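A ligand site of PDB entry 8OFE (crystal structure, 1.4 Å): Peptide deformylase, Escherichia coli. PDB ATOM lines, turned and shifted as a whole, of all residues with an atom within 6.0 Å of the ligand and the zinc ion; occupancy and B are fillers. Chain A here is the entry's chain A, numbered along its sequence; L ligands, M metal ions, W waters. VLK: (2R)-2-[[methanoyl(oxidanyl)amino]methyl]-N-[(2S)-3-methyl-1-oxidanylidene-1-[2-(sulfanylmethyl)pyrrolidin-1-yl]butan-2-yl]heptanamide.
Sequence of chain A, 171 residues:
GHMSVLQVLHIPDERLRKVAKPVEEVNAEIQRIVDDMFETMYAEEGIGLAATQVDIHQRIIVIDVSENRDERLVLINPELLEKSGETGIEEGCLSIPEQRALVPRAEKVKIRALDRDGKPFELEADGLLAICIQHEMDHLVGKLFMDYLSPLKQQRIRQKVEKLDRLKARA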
ATOM      1  N   GLU A  44      13.490 -13.737 -15.093  1.00  0.00           N
ATOM      2  CA  GLU A  44      14.362 -12.854 -15.870  1.00  0.00           C
ATOM      3  C   GLU A  44      15.234 -11.973 -14.993  1.00  0.00           C
ATOM      4  O   GLU A  44      15.944 -11.091 -15.522  1.00  0.00           O
ATOM      5  CB  GLU A  44      13.526 -12.002 -16.823  1.00  0.00           C
ATOM      6  CG  GLU A  44      12.674 -12.860 -17.786  1.00  0.00           C
ATOM      7  CD  GLU A  44      12.987 -12.571 -19.253  1.00  0.00           C
ATOM      8  OE1 GLU A  44      13.322 -11.412 -19.584  1.00  0.00           O
ATOM      9  OE2 GLU A  44      12.928 -13.522 -20.058  1.00  0.00           O
ATOM     10  N   GLU A  45      15.183 -12.183 -13.681  1.00  0.00           N
ATOM     11  CA  GLU A  45      15.978 -11.440 -12.708  1.00  0.00           C
ATOM     12  C   GLU A  45      15.614  -9.956 -12.683  1.00  0.00           C
ATOM     13  O   GLU A  45      16.490  -9.107 -12.465  1.00  0.00           O
ATOM     14  CB  GLU A  45      17.491 -11.668 -12.898  1.00  0.00           C
ATOM     15  CG  GLU A  45      17.862 -13.119 -12.621  1.00  0.00           C
ATOM     16  CD  GLU A  45      19.259 -13.480 -12.947  1.00  0.00           C
ATOM     17  OE1 GLU A  45      20.092 -12.590 -13.188  1.00  0.00           O
ATOM     18  OE2 GLU A  45      19.515 -14.687 -12.951  1.00  0.00           O
ATOM     19  N   GLY A  46      14.359  -9.637 -12.922  1.00  0.00           N
ATOM     20  CA  GLY A  46      13.919  -8.265 -12.883  1.00  0.00           C
ATOM     21  C   GLY A  46      13.405  -7.862 -11.525  1.00  0.00           C
ATOM     22  O   GLY A  46      13.039  -8.704 -10.706  1.00  0.00           O
ATOM     23  N   ILE A  47      13.284  -6.551 -11.305  1.00  0.00           N
ATOM     24  CA  ILE A  47      12.652  -5.993 -10.112  1.00  0.00           C
ATOM     25  C   ILE A  47      11.307  -5.371 -10.429  1.00  0.00           C
ATOM     26  O   ILE A  47      10.607  -4.932  -9.524  1.00  0.00           O
ATOM     27  CB  ILE A  47      13.560  -5.005  -9.360  1.00  0.00           C
ATOM     28  CG1 ILE A  47      13.892  -3.818 -10.265  1.00  0.00           C
ATOM     29  CG2 ILE A  47      14.820  -5.687  -8.889  1.00  0.00           C
ATOM     30  CD1 ILE A  47      14.640  -2.728  -9.515  1.00  0.00           C
ATOM     31  N   GLY A  48      10.928  -5.322 -11.707  1.00  0.00           N
ATOM     32  CA  GLY A  48       9.590  -4.884 -12.058  1.00  0.00           C
ATOM     33  C   GLY A  48       9.260  -5.451 -13.401  1.00  0.00           C
ATOM     34  O   GLY A  48      10.147  -5.861 -14.140  1.00  0.00           O
ATOM     35  N   LEU A  49       7.974  -5.425 -13.738  1.00  0.00           N
ATOM     36  CA  LEU A  49       7.506  -5.871 -15.039  1.00  0.00           C
ATOM     37  C   LEU A  49       6.135  -5.252 -15.259  1.00  0.00           C
ATOM     38  O   LEU A  49       5.292  -5.264 -14.368  1.00  0.00           O
ATOM     39  CB  LEU A  49       7.365  -7.407 -15.087  1.00  0.00           C
ATOM     40  CG  LEU A  49       7.128  -8.033 -16.440  1.00  0.00           C
ATOM     41  CD1 LEU A  49       8.318  -7.894 -17.329  1.00  0.00           C
ATOM     42  CD2 LEU A  49       6.722  -9.513 -16.351  1.00  0.00           C
ATOM     43  N   ALA A  50       5.923  -4.727 -16.470  1.00  0.00           N
ATOM     44  CA  ALA A  50       4.652  -4.144 -16.855  1.00  0.00           C
ATOM     45  C   ALA A  50       3.951  -5.061 -17.843  1.00  0.00           C
ATOM     46  O   ALA A  50       4.600  -5.729 -18.659  1.00  0.00           O
ATOM     47  CB  ALA A  50       4.900  -2.751 -17.480  1.00  0.00           C
ATOM     48  N   GLN A  53       4.892  -5.320 -21.480  1.00  0.00           N
ATOM     49  CA  GLN A  53       6.121  -6.025 -21.879  1.00  0.00           C
ATOM     50  C   GLN A  53       5.868  -7.489 -22.224  1.00  0.00           C
ATOM     51  O   GLN A  53       6.756  -8.142 -22.803  1.00  0.00           O
ATOM     52  CB  GLN A  53       7.180  -5.971 -20.791  1.00  0.00           C
ATOM     53  CG  GLN A  53       7.698  -4.542 -20.484  1.00  0.00           C
ATOM     54  CD  GLN A  53       8.699  -4.587 -19.347  1.00  0.00           C
ATOM     55  OE1 GLN A  53       8.322  -4.533 -18.195  1.00  0.00           O
ATOM     56  NE2 GLN A  53       9.975  -4.712 -19.694  1.00  0.00           N
ATOM     57  N   ILE A  89      19.423   7.057 -11.795  1.00  0.00           N
ATOM     58  CA  ILE A  89      20.395   5.968 -11.745  1.00  0.00           C
ATOM     59  C   ILE A  89      20.525   5.369 -13.132  1.00  0.00           C
ATOM     60  O   ILE A  89      19.724   5.646 -14.025  1.00  0.00           O
ATOM     61  CB  ILE A  89      19.985   4.886 -10.730  1.00  0.00           C
ATOM     62  CG1 ILE A  89      18.689   4.152 -11.163  1.00  0.00           C
ATOM     63  CG2 ILE A  89      19.901   5.512  -9.338  1.00  0.00           C
ATOM     64  CD1 ILE A  89      18.288   2.982 -10.201  1.00  0.00           C
ATOM     65  N   GLU A  90      21.518   4.509 -13.278  1.00  0.00           N
ATOM     66  CA  GLU A  90      21.680   3.726 -14.492  1.00  0.00           C
ATOM     67  C   GLU A  90      20.605   2.672 -14.557  1.00  0.00           C
ATOM     68  O   GLU A  90      20.645   1.689 -13.815  1.00  0.00           O
ATOM     69  CB  GLU A  90      23.054   3.045 -14.494  1.00  0.00           C
ATOM     70  CG  GLU A  90      24.146   4.007 -14.607  1.00  0.00           C
ATOM     71  CD  GLU A  90      24.455   4.402 -16.012  1.00  0.00           C
ATOM     72  OE1 GLU A  90      23.893   3.810 -16.956  1.00  0.00           O
ATOM     73  OE2 GLU A  90      25.303   5.291 -16.168  1.00  0.00           O
ATOM     74  N   GLU A  91      19.604   2.862 -15.406  1.00  0.00           N
ATOM     75  CA  GLU A  91      18.487   1.924 -15.517  1.00  0.00           C
ATOM     76  C   GLU A  91      18.749   0.941 -16.629  1.00  0.00           C
ATOM     77  O   GLU A  91      19.336   1.285 -17.634  1.00  0.00           O
ATOM     78  CB  GLU A  91      17.190   2.668 -15.835  1.00  0.00           C
ATOM     79  CG  GLU A  91      16.737   3.590 -14.764  1.00  0.00           C
ATOM     80  CD  GLU A  91      15.383   4.236 -15.032  1.00  0.00           C
ATOM     81  OE1 GLU A  91      14.520   3.668 -15.782  1.00  0.00           O
ATOM     82  OE2 GLU A  91      15.136   5.294 -14.431  1.00  0.00           O
ATOM     83  N   GLY A  92      18.317  -0.306 -16.423  1.00  0.00           N
ATOM     84  CA  GLY A  92      18.171  -1.283 -17.474  1.00  0.00           C
ATOM     85  C   GLY A  92      16.707  -1.656 -17.652  1.00  0.00           C
ATOM     86  O   GLY A  92      15.841  -1.183 -16.912  1.00  0.00           O
ATOM     87  N   CYS A  93      16.426  -2.450 -18.694  1.00  0.00           N
ATOM     88  CA  CYS A  93      15.058  -2.806 -19.050  1.00  0.00           C
ATOM     89  C   CYS A  93      15.095  -4.191 -19.685  1.00  0.00           C
ATOM     90  O   CYS A  93      15.910  -4.435 -20.573  1.00  0.00           O
ATOM     91  CB  CYS A  93      14.420  -1.784 -20.017  1.00  0.00           C
ATOM     92  SG  CYS A  93      12.704  -2.126 -20.435  1.00  0.00           S
ATOM     93  N   LEU A  94      14.174  -5.072 -19.249  1.00  0.00           N
ATOM     94  CA  LEU A  94      14.123  -6.420 -19.835  1.00  0.00           C
ATOM     95  C   LEU A  94      13.770  -6.381 -21.314  1.00  0.00           C
ATOM     96  O   LEU A  94      14.019  -7.371 -22.026  1.00  0.00           O
ATOM     97  CB  LEU A  94      13.102  -7.284 -19.105  1.00  0.00           C
ATOM     98  CG  LEU A  94      13.481  -7.705 -17.675  1.00  0.00           C
ATOM     99  CD1 LEU A  94      12.327  -8.421 -16.951  1.00  0.00           C
ATOM    100  CD2 LEU A  94      14.747  -8.588 -17.705  1.00  0.00           C
ATOM    101  N   SER A  95      13.132  -5.286 -21.753  1.00  0.00           N
ATOM    102  CA  SER A  95      12.788  -5.128 -23.169  1.00  0.00           C
ATOM    103  C   SER A  95      13.910  -4.507 -23.993  1.00  0.00           C
ATOM    104  O   SER A  95      13.763  -4.405 -25.223  1.00  0.00           O
ATOM    105  CB  SER A  95      11.500  -4.307 -23.328  1.00  0.00           C
ATOM    106  OG  SER A  95      10.417  -4.952 -22.674  1.00  0.00           O
ATOM    107  N   GLN A  99      21.484  -3.111 -22.149  1.00  0.00           N
ATOM    108  CA  GLN A  99      21.756  -1.677 -22.255  1.00  0.00           C
ATOM    109  C   GLN A  99      21.348  -0.970 -20.968  1.00  0.00           C
ATOM    110  O   GLN A  99      20.369  -1.336 -20.316  1.00  0.00           O
ATOM    111  CB  GLN A  99      21.000  -1.109 -23.444  1.00  0.00           C
ATOM    112  CG  GLN A  99      21.113  -1.930 -24.730  1.00  0.00           C
ATOM    113  CD  GLN A  99      22.546  -2.284 -25.097  1.00  0.00           C
ATOM    114  OE1 GLN A  99      23.409  -1.412 -25.207  1.00  0.00           O
ATOM    115  NE2 GLN A  99      22.808  -3.606 -25.260  1.00  0.00           N
ATOM    116  N   LEU A 128      15.086   3.976  -5.037  1.00  0.00           N
ATOM    117  CA  LEU A 128      14.967   2.929  -6.046  1.00  0.00           C
ATOM    118  C   LEU A 128      13.509   2.587  -6.335  1.00  0.00           C
ATOM    119  O   LEU A 128      13.117   2.419  -7.504  1.00  0.00           O
ATOM    120  CB  LEU A 128      15.741   1.690  -5.580  1.00  0.00           C
ATOM    121  CG  LEU A 128      15.605   0.503  -6.561  1.00  0.00           C
ATOM    122  CD1 LEU A 128      16.191   0.772  -7.977  1.00  0.00           C
ATOM    123  CD2 LEU A 128      16.250  -0.736  -5.895  1.00  0.00           C
ATOM    124  N   ILE A 131      11.869   5.148  -8.523  1.00  0.00           N
ATOM    125  CA  ILE A 131      12.399   5.046  -9.873  1.00  0.00           C
ATOM    126  C   ILE A 131      11.735   3.889 -10.612  1.00  0.00           C
ATOM    127  O   ILE A 131      11.268   4.022 -11.761  1.00  0.00           O
ATOM    128  CB  ILE A 131      13.939   4.906  -9.805  1.00  0.00           C
ATOM    129  CG1 ILE A 131      14.564   6.257  -9.345  1.00  0.00           C
ATOM    130  CG2 ILE A 131      14.517   4.478 -11.126  1.00  0.00           C
ATOM    131  CD1 ILE A 131      16.003   6.150  -8.944  1.00  0.00           C
ATOM    132  N   CYS A 132      11.669   2.721  -9.960  1.00  0.00           N
ATOM    133  CA  CYS A 132      11.066   1.574 -10.596  1.00  0.00           C
ATOM    134  C   CYS A 132       9.589   1.806 -10.912  1.00  0.00           C
ATOM    135  O   CYS A 132       9.118   1.445 -12.010  1.00  0.00           O
ATOM    136  CB  CYS A 132      11.271   0.372  -9.656  1.00  0.00           C
ATOM    137  SG  CYS A 132      10.552  -1.150 -10.270  1.00  0.00           S
ATOM    138  N   HIS A 135       9.452   3.928 -14.043  1.00  0.00           N
ATOM    139  CA  HIS A 135       9.828   3.125 -15.190  1.00  0.00           C
ATOM    140  C   HIS A 135       8.677   2.215 -15.640  1.00  0.00           C
ATOM    141  O   HIS A 135       8.354   2.118 -16.828  1.00  0.00           O
ATOM    142  CB  HIS A 135      11.081   2.349 -14.800  1.00  0.00           C
ATOM    143  CG  HIS A 135      11.631   1.420 -15.843  1.00  0.00           C
ATOM    144  ND1 HIS A 135      12.884   1.575 -16.384  1.00  0.00           N
ATOM    145  CD2 HIS A 135      11.117   0.295 -16.394  1.00  0.00           C
ATOM    146  CE1 HIS A 135      13.099   0.599 -17.248  1.00  0.00           C
ATOM    147  NE2 HIS A 135      12.053  -0.193 -17.256  1.00  0.00           N
ATOM    148  N   GLU A 136       8.010   1.546 -14.695  1.00  0.00           N
ATOM    149  CA  GLU A 136       6.945   0.638 -15.069  1.00  0.00           C
ATOM    150  C   GLU A 136       5.704   1.389 -15.546  1.00  0.00           C
ATOM    151  O   GLU A 136       5.051   0.936 -16.488  1.00  0.00           O
ATOM    152  CB  GLU A 136       6.548  -0.266 -13.894  1.00  0.00           C
ATOM    153  CG  GLU A 136       7.730  -1.052 -13.314  1.00  0.00           C
ATOM    154  CD  GLU A 136       8.511  -1.836 -14.336  1.00  0.00           C
ATOM    155  OE1 GLU A 136       7.986  -2.152 -15.425  1.00  0.00           O
ATOM    156  OE2 GLU A 136       9.702  -2.101 -14.042  1.00  0.00           O
ATOM    157  N   HIS A 139       6.006   2.200 -19.074  1.00  0.00           N
ATOM    158  CA  HIS A 139       5.710   1.116 -20.006  1.00  0.00           C
ATOM    159  C   HIS A 139       4.234   1.054 -20.352  1.00  0.00           C
ATOM    160  O   HIS A 139       3.863   0.725 -21.488  1.00  0.00           O
ATOM    161  CB  HIS A 139       6.069  -0.245 -19.399  1.00  0.00           C
ATOM    162  CG  HIS A 139       7.493  -0.645 -19.592  1.00  0.00           C
ATOM    163  ND1 HIS A 139       8.096  -0.733 -20.834  1.00  0.00           N
ATOM    164  CD2 HIS A 139       8.450  -0.990 -18.683  1.00  0.00           C
ATOM    165  CE1 HIS A 139       9.343  -1.139 -20.683  1.00  0.00           C
ATOM    166  NE2 HIS A 139       9.585  -1.281 -19.401  1.00  0.00           N
ATOM    167  N   LEU A 144       9.624   4.079 -23.067  1.00  0.00           N
ATOM    168  CA  LEU A 144      10.822   3.325 -22.715  1.00  0.00           C
ATOM    169  C   LEU A 144      11.871   4.276 -22.178  1.00  0.00           C
ATOM    170  O   LEU A 144      11.904   5.452 -22.549  1.00  0.00           O
ATOM    171  CB  LEU A 144      11.392   2.600 -23.935  1.00  0.00           C
ATOM    172  CG  LEU A 144      10.371   1.639 -24.536  1.00  0.00           C
ATOM    173  CD1 LEU A 144      10.889   1.110 -25.880  1.00  0.00           C
ATOM    174  CD2 LEU A 144      10.089   0.498 -23.564  1.00  0.00           C
ATOM    175  N   PHE A 145      12.798   3.778 -21.365  1.00  0.00           N
ATOM    176  CA  PHE A 145      13.753   4.699 -20.754  1.00  0.00           C
ATOM    177  C   PHE A 145      14.615   5.365 -21.815  1.00  0.00           C
ATOM    178  O   PHE A 145      15.088   6.493 -21.620  1.00  0.00           O
ATOM    179  CB  PHE A 145      14.620   4.031 -19.664  1.00  0.00           C
ATOM    180  CG  PHE A 145      15.766   3.176 -20.172  1.00  0.00           C
ATOM    181  CD1 PHE A 145      16.952   3.754 -20.592  1.00  0.00           C
ATOM    182  CD2 PHE A 145      15.659   1.803 -20.232  1.00  0.00           C
ATOM    183  CE1 PHE A 145      17.998   2.981 -21.041  1.00  0.00           C
ATOM    184  CE2 PHE A 145      16.699   1.027 -20.652  1.00  0.00           C
ATOM    185  CZ  PHE A 145      17.867   1.605 -21.055  1.00  0.00           C
HETATM  186  C1  VLK L   1      15.766   0.528 -12.224  1.00  0.00           C
HETATM  187  C2  VLK L   1      14.411   0.866 -12.815  1.00  0.00           C
HETATM  188  C6  VLK L   1      13.702  -3.577 -15.063  1.00  0.00           C
HETATM  189  C5  VLK L   1      13.046  -2.589 -14.096  1.00  0.00           C
HETATM  190  C4  VLK L   1      14.012  -1.529 -13.600  1.00  0.00           C
HETATM  191  C3  VLK L   1      13.442  -0.309 -12.873  1.00  0.00           C
HETATM  192  C11 VLK L   1      18.261  -3.597 -13.790  1.00  0.00           C
HETATM  193  C10 VLK L   1      17.256  -4.669 -14.202  1.00  0.00           C
HETATM  194  C8  VLK L   1      10.716  -3.479 -16.270  1.00  0.00           C
HETATM  195  C18 VLK L   1      16.888  -6.864 -15.341  1.00  0.00           C
HETATM  196  C17 VLK L   1      17.852  -5.695 -15.189  1.00  0.00           C
HETATM  197  C19 VLK L   1      18.174  -5.085 -16.536  1.00  0.00           C
HETATM  198  C7  VLK L   1      12.749  -4.633 -15.603  1.00  0.00           C
HETATM  199  C9  VLK L   1      14.849  -4.307 -14.373  1.00  0.00           C
HETATM  200  N1  VLK L   1      11.880  -3.944 -16.544  1.00  0.00           N
HETATM  201  N2  VLK L   1      16.083  -3.999 -14.753  1.00  0.00           N
HETATM  202  N3  VLK L   1      19.242  -3.986 -12.943  1.00  0.00           N
HETATM  203  O1  VLK L   1      12.322  -3.626 -17.829  1.00  0.00           O
HETATM  204  O2  VLK L   1      10.179  -2.719 -17.014  1.00  0.00           O
HETATM  205  O3  VLK L   1      14.613  -5.141 -13.521  1.00  0.00           O
HETATM  206  O4  VLK L   1      18.181  -2.446 -14.199  1.00  0.00           O
HETATM  207 ZN    ZN M   1      11.476  -1.838 -18.478  1.00  0.00          ZN
HETATM  208  O   HOH W   1      18.915  -8.311 -12.912  1.00  0.00           O
HETATM  209  O   HOH W   2      19.379  -6.029 -11.358  1.00  0.00           O
HETATM  210  O   HOH W   3      21.792  -5.599 -12.499  1.00  0.00           O
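O2 of the ligand sits close to OE1 of Gln 53, 2.9 Å away. N of Gly 92 sits at hydrogen-bond distance from O4 of the ligand. The backbone NH of Ile 47 sits at hydrogen-bond distance from an oxygen (O3) of the ligand (2.9 Å). The backbone NH (N) of Leu 94 lies close to an oxygen (O1) of the ligand.
OE1 of Glu 136 sits at hydrogen-bond distance from N of Ala 50 (3.5 Å). The side-chain amide oxygen (OE1) of Gln 53 sits at hydrogen-bond distance from the backbone NH (N) of Ala 50, at 3.0 Å. The side-chain sulfur (SG) of Cys 93 lies close to the backbone NH (N) of Ser 95, 3.5 Å away. OE1 of Glu 91 lies within hydrogen-bond range of ND1 of His 135, at 2.7 Å. A ring nitrogen (NE2) of His 139 lies close to the side-chain amide nitrogen of Gln 53, 3.5 Å away. The side-chain amide nitrogen of Gln 53 lies within hydrogen-bond range of the side-chain hydroxyl of Ser 95, at 3.0 Å.
The side-chain carboxylate (OE1) of Glu 136 sits close to an oxygen (O2) of the ligand, 2.8 Å away. O of Glu 45 touches C18 of the ligand (3.7 Å). Gly 46 touches the ligand (CA to O3, 3.3 Å). Gly 48 touches the ligand (O to C7, 3.2 Å). Ile 131 touches the ligand. CA of Cys 132 touches C3 of the ligand, 3.8 Å away. Hydrophobic or aromatic side chains within 4 Å of the ligand: Ile 47, Leu 94, Ile 131, His 135 and His 139. Of the 24 residues printed, 13 come within 4 Å of the ligand.
Merely in contact with the zinc ion: Gln 53. Four residues have an atom within 4 Å of the zinc ion: Gln 53, Cys 93, His 135 and His 139.
An oxygen (O1) of the ligand is bound to the zinc ion (2.1 Å). A ring nitrogen (NE2) of His 135 binds the zinc ion (2.1 Å). O2 of the ligand is bound to the zinc ion (2.1 Å). NE2 of His 139 is bound to the zinc ion. The side-chain sulfur (SG) of Cys 93 is bound to the zinc ion, at 2.3 Å.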
